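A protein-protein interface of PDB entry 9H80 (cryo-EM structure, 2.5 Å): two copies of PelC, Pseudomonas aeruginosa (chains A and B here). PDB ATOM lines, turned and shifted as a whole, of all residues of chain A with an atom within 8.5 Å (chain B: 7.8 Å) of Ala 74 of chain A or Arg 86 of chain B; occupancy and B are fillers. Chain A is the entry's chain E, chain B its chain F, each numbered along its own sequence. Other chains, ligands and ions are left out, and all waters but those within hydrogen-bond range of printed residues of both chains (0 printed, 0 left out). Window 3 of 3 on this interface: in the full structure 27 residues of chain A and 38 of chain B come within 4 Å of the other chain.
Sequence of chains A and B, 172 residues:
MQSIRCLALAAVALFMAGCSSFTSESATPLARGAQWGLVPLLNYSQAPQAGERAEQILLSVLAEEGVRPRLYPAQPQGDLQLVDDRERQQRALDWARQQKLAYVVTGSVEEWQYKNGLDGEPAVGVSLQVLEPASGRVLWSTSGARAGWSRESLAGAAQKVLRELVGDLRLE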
ATOM      1  N   LEU A  38      -6.002   9.780 -25.782  1.00  0.00           N
ATOM      2  CA  LEU A  38      -7.099   9.566 -24.839  1.00  0.00           C
ATOM      3  C   LEU A  38      -7.164   8.083 -24.507  1.00  0.00           C
ATOM      4  O   LEU A  38      -7.485   7.265 -25.374  1.00  0.00           O
ATOM      5  CB  LEU A  38      -8.425  10.060 -25.420  1.00  0.00           C
ATOM      6  CG  LEU A  38      -9.700   9.836 -24.601  1.00  0.00           C
ATOM      7  CD1 LEU A  38      -9.574  10.386 -23.193  1.00  0.00           C
ATOM      8  CD2 LEU A  38     -10.887  10.471 -25.306  1.00  0.00           C
ATOM      9  N   GLN A  49     -19.762   0.419 -16.509  1.00  0.00           N
ATOM     10  CA  GLN A  49     -19.569   1.114 -17.783  1.00  0.00           C
ATOM     11  C   GLN A  49     -19.672   2.632 -17.630  1.00  0.00           C
ATOM     12  O   GLN A  49     -19.972   3.346 -18.586  1.00  0.00           O
ATOM     13  CB  GLN A  49     -20.559   0.613 -18.837  1.00  0.00           C
ATOM     14  CG  GLN A  49     -20.344  -0.827 -19.248  1.00  0.00           C
ATOM     15  CD  GLN A  49     -21.110  -1.192 -20.499  1.00  0.00           C
ATOM     16  OE1 GLN A  49     -22.333  -1.074 -20.547  1.00  0.00           O
ATOM     17  NE2 GLN A  49     -20.396  -1.641 -21.523  1.00  0.00           N
ATOM     18  N   GLU A  52     -16.580   4.327 -19.630  1.00  0.00           N
ATOM     19  CA  GLU A  52     -16.804   4.483 -21.063  1.00  0.00           C
ATOM     20  C   GLU A  52     -17.770   5.621 -21.374  1.00  0.00           C
ATOM     21  O   GLU A  52     -17.540   6.384 -22.321  1.00  0.00           O
ATOM     22  CB  GLU A  52     -17.326   3.175 -21.650  1.00  0.00           C
ATOM     23  CG  GLU A  52     -16.377   2.007 -21.470  1.00  0.00           C
ATOM     24  CD  GLU A  52     -16.759   1.118 -20.306  1.00  0.00           C
ATOM     25  OE1 GLU A  52     -17.379   0.062 -20.543  1.00  0.00           O
ATOM     26  OE2 GLU A  52     -16.440   1.475 -19.152  1.00  0.00           O
ATOM     27  N   GLU A  55     -15.897   8.733 -20.946  1.00  0.00           N
ATOM     28  CA  GLU A  55     -14.994   8.959 -22.069  1.00  0.00           C
ATOM     29  C   GLU A  55     -15.733   9.507 -23.280  1.00  0.00           C
ATOM     30  O   GLU A  55     -15.212  10.375 -23.983  1.00  0.00           O
ATOM     31  CB  GLU A  55     -14.265   7.673 -22.449  1.00  0.00           C
ATOM     32  CG  GLU A  55     -13.396   7.839 -23.695  1.00  0.00           C
ATOM     33  CD  GLU A  55     -12.574   6.621 -24.002  1.00  0.00           C
ATOM     34  OE1 GLU A  55     -12.446   5.737 -23.126  1.00  0.00           O
ATOM     35  OE2 GLU A  55     -12.071   6.545 -25.141  1.00  0.00           O
ATOM     36  N   GLN A  56     -16.919   8.978 -23.579  1.00  0.00           N
ATOM     37  CA  GLN A  56     -17.658   9.478 -24.736  1.00  0.00           C
ATOM     38  C   GLN A  56     -18.035  10.943 -24.542  1.00  0.00           C
ATOM     39  O   GLN A  56     -17.848  11.779 -25.441  1.00  0.00           O
ATOM     40  CB  GLN A  56     -18.906   8.626 -24.976  1.00  0.00           C
ATOM     41  CG  GLN A  56     -18.631   7.186 -25.401  1.00  0.00           C
ATOM     42  CD  GLN A  56     -17.748   7.081 -26.629  1.00  0.00           C
ATOM     43  OE1 GLN A  56     -18.111   7.541 -27.710  1.00  0.00           O
ATOM     44  NE2 GLN A  56     -16.578   6.476 -26.465  1.00  0.00           N
ATOM     45  N   LEU A  59     -14.936  13.040 -24.915  1.00  0.00           N
ATOM     46  CA  LEU A  59     -14.562  13.233 -26.309  1.00  0.00           C
ATOM     47  C   LEU A  59     -15.420  14.316 -26.941  1.00  0.00           C
ATOM     48  O   LEU A  59     -14.921  15.146 -27.710  1.00  0.00           O
ATOM     49  CB  LEU A  59     -14.697  11.917 -27.076  1.00  0.00           C
ATOM     50  CG  LEU A  59     -14.326  11.928 -28.564  1.00  0.00           C
ATOM     51  CD1 LEU A  59     -12.842  12.198 -28.746  1.00  0.00           C
ATOM     52  CD2 LEU A  59     -14.721  10.621 -29.228  1.00  0.00           C
ATOM     53  N   LEU A  71      -7.845   8.336 -30.237  1.00  0.00           N
ATOM     54  CA  LEU A  71      -8.393   7.369 -29.302  1.00  0.00           C
ATOM     55  C   LEU A  71      -7.537   6.110 -29.287  1.00  0.00           C
ATOM     56  O   LEU A  71      -6.981   5.701 -30.309  1.00  0.00           O
ATOM     57  CB  LEU A  71      -9.837   7.012 -29.664  1.00  0.00           C
ATOM     58  CG  LEU A  71     -10.720   8.112 -30.260  1.00  0.00           C
ATOM     59  CD1 LEU A  71     -12.093   7.564 -30.599  1.00  0.00           C
ATOM     60  CD2 LEU A  71     -10.831   9.296 -29.314  1.00  0.00           C
ATOM     61  N   TYR A  72      -7.426   5.505 -28.108  1.00  0.00           N
ATOM     62  CA  TYR A  72      -6.686   4.260 -27.988  1.00  0.00           C
ATOM     63  C   TYR A  72      -7.345   3.188 -28.859  1.00  0.00           C
ATOM     64  O   TYR A  72      -8.567   3.192 -29.040  1.00  0.00           O
ATOM     65  CB  TYR A  72      -6.642   3.758 -26.543  1.00  0.00           C
ATOM     66  CG  TYR A  72      -7.992   3.426 -25.922  1.00  0.00           C
ATOM     67  CD1 TYR A  72      -8.919   4.408 -25.610  1.00  0.00           C
ATOM     68  CD2 TYR A  72      -8.306   2.116 -25.589  1.00  0.00           C
ATOM     69  CE1 TYR A  72     -10.128   4.091 -25.038  1.00  0.00           C
ATOM     70  CE2 TYR A  72      -9.522   1.791 -25.021  1.00  0.00           C
ATOM     71  CZ  TYR A  72     -10.427   2.787 -24.744  1.00  0.00           C
ATOM     72  OH  TYR A  72     -11.639   2.487 -24.166  1.00  0.00           O
ATOM     73  N   PRO A  73      -6.570   2.256 -29.410  1.00  0.00           N
ATOM     74  CA  PRO A  73      -7.173   1.192 -30.216  1.00  0.00           C
ATOM     75  C   PRO A  73      -7.965   0.222 -29.355  1.00  0.00           C
ATOM     76  O   PRO A  73      -7.724   0.063 -28.157  1.00  0.00           O
ATOM     77  CB  PRO A  73      -5.964   0.505 -30.855  1.00  0.00           C
ATOM     78  CG  PRO A  73      -4.887   0.692 -29.859  1.00  0.00           C
ATOM     79  CD  PRO A  73      -5.118   2.052 -29.259  1.00  0.00           C
ATOM     80  N   ALA A  74      -8.927  -0.436 -29.994  1.00  0.00           N
ATOM     81  CA  ALA A  74      -9.737  -1.455 -29.332  1.00  0.00           C
ATOM     82  C   ALA A  74      -8.866  -2.685 -29.118  1.00  0.00           C
ATOM     83  O   ALA A  74      -8.630  -3.463 -30.044  1.00  0.00           O
ATOM     84  CB  ALA A  74     -10.971  -1.782 -30.163  1.00  0.00           C
ATOM     85  N   GLN A  75      -8.379  -2.858 -27.899  1.00  0.00           N
ATOM     86  CA  GLN A  75      -7.514  -3.990 -27.591  1.00  0.00           C
ATOM     87  C   GLN A  75      -8.344  -5.270 -27.550  1.00  0.00           C
ATOM     88  O   GLN A  75      -9.316  -5.334 -26.786  1.00  0.00           O
ATOM     89  CB  GLN A  75      -6.814  -3.769 -26.255  1.00  0.00           C
ATOM     90  CG  GLN A  75      -5.817  -2.612 -26.261  1.00  0.00           C
ATOM     91  CD  GLN A  75      -6.135  -1.536 -25.233  1.00  0.00           C
ATOM     92  OE1 GLN A  75      -6.685  -1.814 -24.166  1.00  0.00           O
ATOM     93  NE2 GLN A  75      -5.790  -0.295 -25.555  1.00  0.00           N
ATOM     94  N   PRO A  76      -8.018  -6.304 -28.332  1.00  0.00           N
ATOM     95  CA  PRO A  76      -8.838  -7.527 -28.295  1.00  0.00           C
ATOM     96  C   PRO A  76      -8.629  -8.276 -26.986  1.00  0.00           C
ATOM     97  O   PRO A  76      -7.495  -8.522 -26.573  1.00  0.00           O
ATOM     98  CB  PRO A  76      -8.337  -8.331 -29.498  1.00  0.00           C
ATOM     99  CG  PRO A  76      -6.942  -7.881 -29.694  1.00  0.00           C
ATOM    100  CD  PRO A  76      -6.891  -6.440 -29.274  1.00  0.00           C
ATOM    101  N   GLN A  77      -9.736  -8.636 -26.335  1.00  0.00           N
ATOM    102  CA  GLN A  77      -9.710  -9.337 -25.060  1.00  0.00           C
ATOM    103  C   GLN A  77     -10.782 -10.414 -25.045  1.00  0.00           C
ATOM    104  O   GLN A  77     -11.896 -10.202 -25.535  1.00  0.00           O
ATOM    105  CB  GLN A  77      -9.933  -8.370 -23.893  1.00  0.00           C
ATOM    106  CG  GLN A  77      -8.747  -7.449 -23.621  1.00  0.00           C
ATOM    107  CD  GLN A  77      -9.138  -5.994 -23.408  1.00  0.00           C
ATOM    108  OE1 GLN A  77     -10.312  -5.662 -23.233  1.00  0.00           O
ATOM    109  NE2 GLN A  77      -8.146  -5.116 -23.437  1.00  0.00           N
ATOM    110  N   ARG A  88      -5.650  -1.991 -18.169  1.00  0.00           N
ATOM    111  CA  ARG A  88      -6.009  -1.454 -19.477  1.00  0.00           C
ATOM    112  C   ARG A  88      -5.416  -0.067 -19.678  1.00  0.00           C
ATOM    113  O   ARG A  88      -4.952   0.269 -20.775  1.00  0.00           O
ATOM    114  CB  ARG A  88      -7.529  -1.393 -19.619  1.00  0.00           C
ATOM    115  CG  ARG A  88      -8.206  -2.681 -20.048  1.00  0.00           C
ATOM    116  CD  ARG A  88      -8.790  -2.584 -21.463  1.00  0.00           C
ATOM    117  NE  ARG A  88      -9.666  -1.435 -21.678  1.00  0.00           N
ATOM    118  CZ  ARG A  88     -10.784  -1.175 -21.010  1.00  0.00           C
ATOM    119  NH1 ARG A  88     -11.279  -2.021 -20.122  1.00  0.00           N
ATOM    120  NH2 ARG A  88     -11.433  -0.039 -21.250  1.00  0.00           N
ATOM    121  N   ARG A  91      -1.759  -0.566 -20.565  1.00  0.00           N
ATOM    122  CA  ARG A  91      -1.614  -1.053 -21.934  1.00  0.00           C
ATOM    123  C   ARG A  91      -2.006  -0.013 -22.974  1.00  0.00           C
ATOM    124  O   ARG A  91      -1.574  -0.129 -24.125  1.00  0.00           O
ATOM    125  CB  ARG A  91      -2.417  -2.339 -22.145  1.00  0.00           C
ATOM    126  CG  ARG A  91      -2.066  -3.453 -21.151  1.00  0.00           C
ATOM    127  CD  ARG A  91      -2.910  -4.720 -21.302  1.00  0.00           C
ATOM    128  NE  ARG A  91      -3.566  -4.854 -22.598  1.00  0.00           N
ATOM    129  CZ  ARG A  91      -4.498  -5.760 -22.873  1.00  0.00           C
ATOM    130  NH1 ARG A  91      -4.929  -6.615 -21.959  1.00  0.00           N
ATOM    131  NH2 ARG A  91      -5.003  -5.813 -24.102  1.00  0.00           N
ATOM    132  N   TRP A  95       0.765   2.222 -25.720  1.00  0.00           N
ATOM    133  CA  TRP A  95       0.418   2.599 -27.089  1.00  0.00           C
ATOM    134  C   TRP A  95       0.647   4.086 -27.312  1.00  0.00           C
ATOM    135  O   TRP A  95       1.186   4.492 -28.348  1.00  0.00           O
ATOM    136  CB  TRP A  95      -1.036   2.242 -27.398  1.00  0.00           C
ATOM    137  CG  TRP A  95      -1.633   3.091 -28.502  1.00  0.00           C
ATOM    138  CD1 TRP A  95      -1.573   2.842 -29.843  1.00  0.00           C
ATOM    139  CD2 TRP A  95      -2.387   4.306 -28.356  1.00  0.00           C
ATOM    140  NE1 TRP A  95      -2.229   3.829 -30.537  1.00  0.00           N
ATOM    141  CE2 TRP A  95      -2.735   4.739 -29.650  1.00  0.00           C
ATOM    142  CE3 TRP A  95      -2.789   5.071 -27.257  1.00  0.00           C
ATOM    143  CZ2 TRP A  95      -3.473   5.900 -29.875  1.00  0.00           C
ATOM    144  CZ3 TRP A  95      -3.520   6.226 -27.485  1.00  0.00           C
ATOM    145  CH2 TRP A  95      -3.853   6.628 -28.783  1.00  0.00           C
ATOM    146  N   PRO B  40     -23.603   0.588 -36.135  1.00  0.00           N
ATOM    147  CA  PRO B  40     -24.382   0.527 -34.894  1.00  0.00           C
ATOM    148  C   PRO B  40     -23.781   1.373 -33.783  1.00  0.00           C
ATOM    149  O   PRO B  40     -22.565   1.532 -33.670  1.00  0.00           O
ATOM    150  CB  PRO B  40     -24.353  -0.961 -34.531  1.00  0.00           C
ATOM    151  CG  PRO B  40     -23.122  -1.475 -35.157  1.00  0.00           C
ATOM    152  CD  PRO B  40     -22.950  -0.700 -36.429  1.00  0.00           C
ATOM    153  N   LEU B  41     -24.667   1.923 -32.959  1.00  0.00           N
ATOM    154  CA  LEU B  41     -24.256   2.682 -31.792  1.00  0.00           C
ATOM    155  C   LEU B  41     -23.796   1.740 -30.684  1.00  0.00           C
ATOM    156  O   LEU B  41     -24.172   0.567 -30.633  1.00  0.00           O
ATOM    157  CB  LEU B  41     -25.404   3.558 -31.289  1.00  0.00           C
ATOM    158  CG  LEU B  41     -25.614   4.891 -32.007  1.00  0.00           C
ATOM    159  CD1 LEU B  41     -26.108   4.680 -33.425  1.00  0.00           C
ATOM    160  CD2 LEU B  41     -26.591   5.751 -31.228  1.00  0.00           C
ATOM    161  N   LEU B  42     -22.971   2.272 -29.788  1.00  0.00           N
ATOM    162  CA  LEU B  42     -22.472   1.529 -28.639  1.00  0.00           C
ATOM    163  C   LEU B  42     -23.357   1.820 -27.438  1.00  0.00           C
ATOM    164  O   LEU B  42     -23.542   2.983 -27.065  1.00  0.00           O
ATOM    165  CB  LEU B  42     -21.023   1.904 -28.330  1.00  0.00           C
ATOM    166  CG  LEU B  42     -20.044   1.862 -29.504  1.00  0.00           C
ATOM    167  CD1 LEU B  42     -18.687   2.377 -29.073  1.00  0.00           C
ATOM    168  CD2 LEU B  42     -19.931   0.456 -30.060  1.00  0.00           C
ATOM    169  N   ASN B  43     -23.895   0.769 -26.833  1.00  0.00           N
ATOM    170  CA  ASN B  43     -24.812   0.895 -25.705  1.00  0.00           C
ATOM    171  C   ASN B  43     -24.015   0.749 -24.415  1.00  0.00           C
ATOM    172  O   ASN B  43     -23.786  -0.363 -23.936  1.00  0.00           O
ATOM    173  CB  ASN B  43     -25.922  -0.145 -25.793  1.00  0.00           C
ATOM    174  CG  ASN B  43     -27.042   0.117 -24.807  1.00  0.00           C
ATOM    175  OD1 ASN B  43     -27.137   1.198 -24.232  1.00  0.00           O
ATOM    176  ND2 ASN B  43     -27.892  -0.879 -24.602  1.00  0.00           N
ATOM    177  N   TYR B  44     -23.590   1.880 -23.854  1.00  0.00           N
ATOM    178  CA  TYR B  44     -22.995   1.912 -22.526  1.00  0.00           C
ATOM    179  C   TYR B  44     -24.024   2.151 -21.433  1.00  0.00           C
ATOM    180  O   TYR B  44     -23.691   2.019 -20.252  1.00  0.00           O
ATOM    181  CB  TYR B  44     -21.908   2.991 -22.454  1.00  0.00           C
ATOM    182  CG  TYR B  44     -20.719   2.722 -23.348  1.00  0.00           C
ATOM    183  CD1 TYR B  44     -20.073   1.494 -23.328  1.00  0.00           C
ATOM    184  CD2 TYR B  44     -20.249   3.693 -24.218  1.00  0.00           C
ATOM    185  CE1 TYR B  44     -18.991   1.244 -24.143  1.00  0.00           C
ATOM    186  CE2 TYR B  44     -19.168   3.449 -25.038  1.00  0.00           C
ATOM    187  CZ  TYR B  44     -18.543   2.224 -24.996  1.00  0.00           C
ATOM    188  OH  TYR B  44     -17.463   1.976 -25.810  1.00  0.00           O
ATOM    189  N   VAL B  83     -20.807 -11.175 -27.602  1.00  0.00           N
ATOM    190  CA  VAL B  83     -20.275 -10.396 -28.716  1.00  0.00           C
ATOM    191  C   VAL B  83     -20.123  -8.951 -28.263  1.00  0.00           C
ATOM    192  O   VAL B  83     -21.104  -8.304 -27.878  1.00  0.00           O
ATOM    193  CB  VAL B  83     -21.182 -10.497 -29.951  1.00  0.00           C
ATOM    194  CG1 VAL B  83     -20.712  -9.540 -31.038  1.00  0.00           C
ATOM    195  CG2 VAL B  83     -21.214 -11.927 -30.472  1.00  0.00           C
ATOM    196  N   ASP B  84     -18.895  -8.442 -28.309  1.00  0.00           N
ATOM    197  CA  ASP B  84     -18.634  -7.072 -27.895  1.00  0.00           C
ATOM    198  C   ASP B  84     -19.255  -6.091 -28.882  1.00  0.00           C
ATOM    199  O   ASP B  84     -19.248  -6.315 -30.095  1.00  0.00           O
ATOM    200  CB  ASP B  84     -17.126  -6.835 -27.789  1.00  0.00           C
ATOM    201  CG  ASP B  84     -16.782  -5.493 -27.173  1.00  0.00           C
ATOM    202  OD1 ASP B  84     -17.132  -4.450 -27.766  1.00  0.00           O
ATOM    203  OD2 ASP B  84     -16.156  -5.479 -26.093  1.00  0.00           O
ATOM    204  N   ASP B  85     -19.800  -4.994 -28.350  1.00  0.00           N
ATOM    205  CA  ASP B  85     -20.369  -3.961 -29.212  1.00  0.00           C
ATOM    206  C   ASP B  85     -19.293  -3.307 -30.071  1.00  0.00           C
ATOM    207  O   ASP B  85     -19.505  -3.057 -31.265  1.00  0.00           O
ATOM    208  CB  ASP B  85     -21.086  -2.908 -28.366  1.00  0.00           C
ATOM    209  CG  ASP B  85     -22.579  -3.147 -28.281  1.00  0.00           C
ATOM    210  OD1 ASP B  85     -22.989  -4.320 -28.159  1.00  0.00           O
ATOM    211  OD2 ASP B  85     -23.344  -2.162 -28.336  1.00  0.00           O
ATOM    212  N   ARG B  86     -18.132  -3.020 -29.477  1.00  0.00           N
ATOM    213  CA  ARG B  86     -17.058  -2.384 -30.231  1.00  0.00           C
ATOM    214  C   ARG B  86     -16.564  -3.280 -31.357  1.00  0.00           C
ATOM    215  O   ARG B  86     -16.144  -2.780 -32.405  1.00  0.00           O
ATOM    216  CB  ARG B  86     -15.902  -2.013 -29.298  1.00  0.00           C
ATOM    217  CG  ARG B  86     -15.409  -0.584 -29.465  1.00  0.00           C
ATOM    218  CD  ARG B  86     -14.528  -0.160 -28.302  1.00  0.00           C
ATOM    219  NE  ARG B  86     -13.470   0.754 -28.720  1.00  0.00           N
ATOM    220  CZ  ARG B  86     -13.592   2.074 -28.808  1.00  0.00           C
ATOM    221  NH1 ARG B  86     -14.732   2.689 -28.537  1.00  0.00           N
ATOM    222  NH2 ARG B  86     -12.540   2.796 -29.183  1.00  0.00           N
ATOM    223  N   GLU B  87     -16.616  -4.600 -31.171  1.00  0.00           N
ATOM    224  CA  GLU B  87     -16.273  -5.513 -32.255  1.00  0.00           C
ATOM    225  C   GLU B  87     -17.191  -5.301 -33.453  1.00  0.00           C
ATOM    226  O   GLU B  87     -16.729  -5.152 -34.592  1.00  0.00           O
ATOM    227  CB  GLU B  87     -16.352  -6.961 -31.767  1.00  0.00           C
ATOM    228  CG  GLU B  87     -15.153  -7.416 -30.952  1.00  0.00           C
ATOM    229  CD  GLU B  87     -15.360  -8.783 -30.326  1.00  0.00           C
ATOM    230  OE1 GLU B  87     -16.462  -9.351 -30.481  1.00  0.00           O
ATOM    231  OE2 GLU B  87     -14.419  -9.291 -29.680  1.00  0.00           O
ATOM    232  N   ARG B  88     -18.505  -5.278 -33.208  1.00  0.00           N
ATOM    233  CA  ARG B  88     -19.456  -5.078 -34.296  1.00  0.00           C
ATOM    234  C   ARG B  88     -19.262  -3.718 -34.945  1.00  0.00           C
ATOM    235  O   ARG B  88     -19.355  -3.588 -36.171  1.00  0.00           O
ATOM    236  CB  ARG B  88     -20.890  -5.221 -33.784  1.00  0.00           C
ATOM    237  CG  ARG B  88     -21.151  -6.473 -32.970  1.00  0.00           C
ATOM    238  CD  ARG B  88     -22.642  -6.699 -32.778  1.00  0.00           C
ATOM    239  NE  ARG B  88     -23.270  -5.589 -32.064  1.00  0.00           N
ATOM    240  CZ  ARG B  88     -24.264  -4.828 -32.513  1.00  0.00           C
ATOM    241  NH1 ARG B  88     -24.810  -5.012 -33.707  1.00  0.00           N
ATOM    242  NH2 ARG B  88     -24.727  -3.849 -31.740  1.00  0.00           N
ATOM    243  N   GLN B  89     -18.993  -2.690 -34.139  1.00  0.00           N
ATOM    244  CA  GLN B  89     -18.744  -1.370 -34.709  1.00  0.00           C
ATOM    245  C   GLN B  89     -17.502  -1.383 -35.591  1.00  0.00           C
ATOM    246  O   GLN B  89     -17.471  -0.732 -36.642  1.00  0.00           O
ATOM    247  CB  GLN B  89     -18.603  -0.332 -33.595  1.00  0.00           C
ATOM    248  CG  GLN B  89     -18.814   1.093 -34.071  1.00  0.00           C
ATOM    249  CD  GLN B  89     -18.518   2.121 -33.003  1.00  0.00           C
ATOM    250  OE1 GLN B  89     -19.398   2.872 -32.587  1.00  0.00           O
ATOM    251  NE2 GLN B  89     -17.268   2.166 -32.555  1.00  0.00           N
ATOM    252  N   GLN B  90     -16.468  -2.121 -35.186  1.00  0.00           N
ATOM    253  CA  GLN B  90     -15.245  -2.182 -35.979  1.00  0.00           C
ATOM    254  C   GLN B  90     -15.488  -2.907 -37.299  1.00  0.00           C
ATOM    255  O   GLN B  90     -14.993  -2.486 -38.353  1.00  0.00           O
ATOM    256  CB  GLN B  90     -14.139  -2.865 -35.172  1.00  0.00           C
ATOM    257  CG  GLN B  90     -12.826  -3.062 -35.921  1.00  0.00           C
ATOM    258  CD  GLN B  90     -12.325  -1.791 -36.579  1.00  0.00           C
ATOM    259  OE1 GLN B  90     -12.088  -0.785 -35.913  1.00  0.00           O
ATOM    260  NE2 GLN B  90     -12.160  -1.832 -37.896  1.00  0.00           N
ATOM    261  N   ARG B  91     -16.253  -4.000 -37.264  1.00  0.00           N
ATOM    262  CA  ARG B  91     -16.588  -4.684 -38.513  1.00  0.00           C
ATOM    263  C   ARG B  91     -17.425  -3.789 -39.418  1.00  0.00           C
ATOM    264  O   ARG B  91     -17.252  -3.793 -40.643  1.00  0.00           O
ATOM    265  CB  ARG B  91     -17.326  -5.998 -38.247  1.00  0.00           C
ATOM    266  CG  ARG B  91     -16.694  -6.901 -37.204  1.00  0.00           C
ATOM    267  CD  ARG B  91     -16.946  -8.413 -37.390  1.00  0.00           C
ATOM    268  NE  ARG B  91     -18.322  -8.832 -37.119  1.00  0.00           N
ATOM    269  CZ  ARG B  91     -19.387  -8.578 -37.868  1.00  0.00           C
ATOM    270  NH1 ARG B  91     -19.281  -8.163 -39.119  1.00  0.00           N
ATOM    271  NH2 ARG B  91     -20.598  -8.804 -37.367  1.00  0.00           N
ATOM    272  N   ALA B  92     -18.348  -3.021 -38.838  1.00  0.00           N
ATOM    273  CA  ALA B  92     -19.151  -2.109 -39.644  1.00  0.00           C
ATOM    274  C   ALA B  92     -18.287  -1.017 -40.266  1.00  0.00           C
ATOM    275  O   ALA B  92     -18.501  -0.625 -41.417  1.00  0.00           O
ATOM    276  CB  ALA B  92     -20.263  -1.504 -38.792  1.00  0.00           C
ATOM    277  N   LEU B  93     -17.307  -0.510 -39.514  1.00  0.00           N
ATOM    278  CA  LEU B  93     -16.371   0.453 -40.087  1.00  0.00           C
ATOM    279  C   LEU B  93     -15.557  -0.170 -41.211  1.00  0.00           C
ATOM    280  O   LEU B  93     -15.270   0.496 -42.212  1.00  0.00           O
ATOM    281  CB  LEU B  93     -15.440   1.002 -39.002  1.00  0.00           C
ATOM    282  CG  LEU B  93     -15.807   2.318 -38.298  1.00  0.00           C
ATOM    283  CD1 LEU B  93     -16.029   3.462 -39.284  1.00  0.00           C
ATOM    284  CD2 LEU B  93     -17.030   2.135 -37.415  1.00  0.00           C
ATOM    285  N   GLN B 129     -21.308  10.866 -33.430  1.00  0.00           N
ATOM    286  CA  GLN B 129     -19.983  11.028 -34.011  1.00  0.00           C
ATOM    287  C   GLN B 129     -20.027  10.719 -35.498  1.00  0.00           C
ATOM    288  O   GLN B 129     -20.784   9.848 -35.937  1.00  0.00           O
ATOM    289  CB  GLN B 129     -18.957  10.116 -33.332  1.00  0.00           C
ATOM    290  CG  GLN B 129     -18.688  10.443 -31.881  1.00  0.00           C
ATOM    291  CD  GLN B 129     -18.148   9.253 -31.121  1.00  0.00           C
ATOM    292  OE1 GLN B 129     -17.114   8.690 -31.483  1.00  0.00           O
ATOM    293  NE2 GLN B 129     -18.846   8.857 -30.063  1.00  0.00           N
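Positions printed for both chains: 88 and 91.
OE1 of Gln 49 of chain A touches O of Asn 43 of chain B (3.8 Å). Tyr 44 of chain B touches Glu 52 of chain A (CE1 to CB, 3.6 Å). CG of Gln 56 of chain A touches CE2 of Tyr 44 of chain B, 3.8 Å away. Leu 59 of chain A touches Gln 129 of chain B. NH2 of Arg 86 of chain B touches O of Tyr 72 of chain A, 3.995 Å away. Arg 86 of chain B touches Ala 74 of chain A (NE to CB, 3.8 Å).
The side-chain amide oxygen (OE1) of Gln 49 of chain A lies close to the backbone carbonyl oxygen (O) of Tyr 44 of chain B, at 3.4 Å. OE1 of Gln 56 of chain A sits at hydrogen-bond distance from NE2 of Gln 129 of chain B, at 2.8 Å.
Along chain A the printed residues that touch a printed residue of chain B span positions 49 to 74. Hydrophobic or aromatic side chains of chain B that line the printed part of chain A: Tyr 44. Along chain B the printed residues that touch a printed residue of chain A span positions 43 to 129. Among the printed residues, no Asp or Glu carboxylate lies within 4 Å of a Lys or Arg side-chain nitrogen of the other chain.
The backbone carbonyl oxygen (O) of Leu 38 of chain A sits close to the backbone NH (N) of Tyr 72 of chain A, 3.3 Å away. The backbone NH of Asn 43 of chain B lies within hydrogen-bond range of the side-chain carboxylate of Asp 85 of chain B, at 3.3 Å. The side-chain carboxylate of Asp 84 of chain B is in hydrogen-bond range of the backbone NH of Arg 86 of chain B (2.4 Å).
Ala 74 of chain A touches one residue of chain B. Of the printed residues of chain A, Arg 86 of chain B touches Tyr 72 (3.995 Å) and Ala 74 (3.8 Å). Printed residues of chain A within 4 Å of Gln 129 of chain B: Gln 56 and Leu 59. Of the printed residues of chain B, Tyr 72 of chain A touches Arg 86 (3.995 Å). Of the printed residues of chain B, Glu 52 of chain A touches Tyr 44. The nearest printed residue of chain A that does not touch Arg 86 of chain B is Gln 56 of chain A (4.7 Å).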
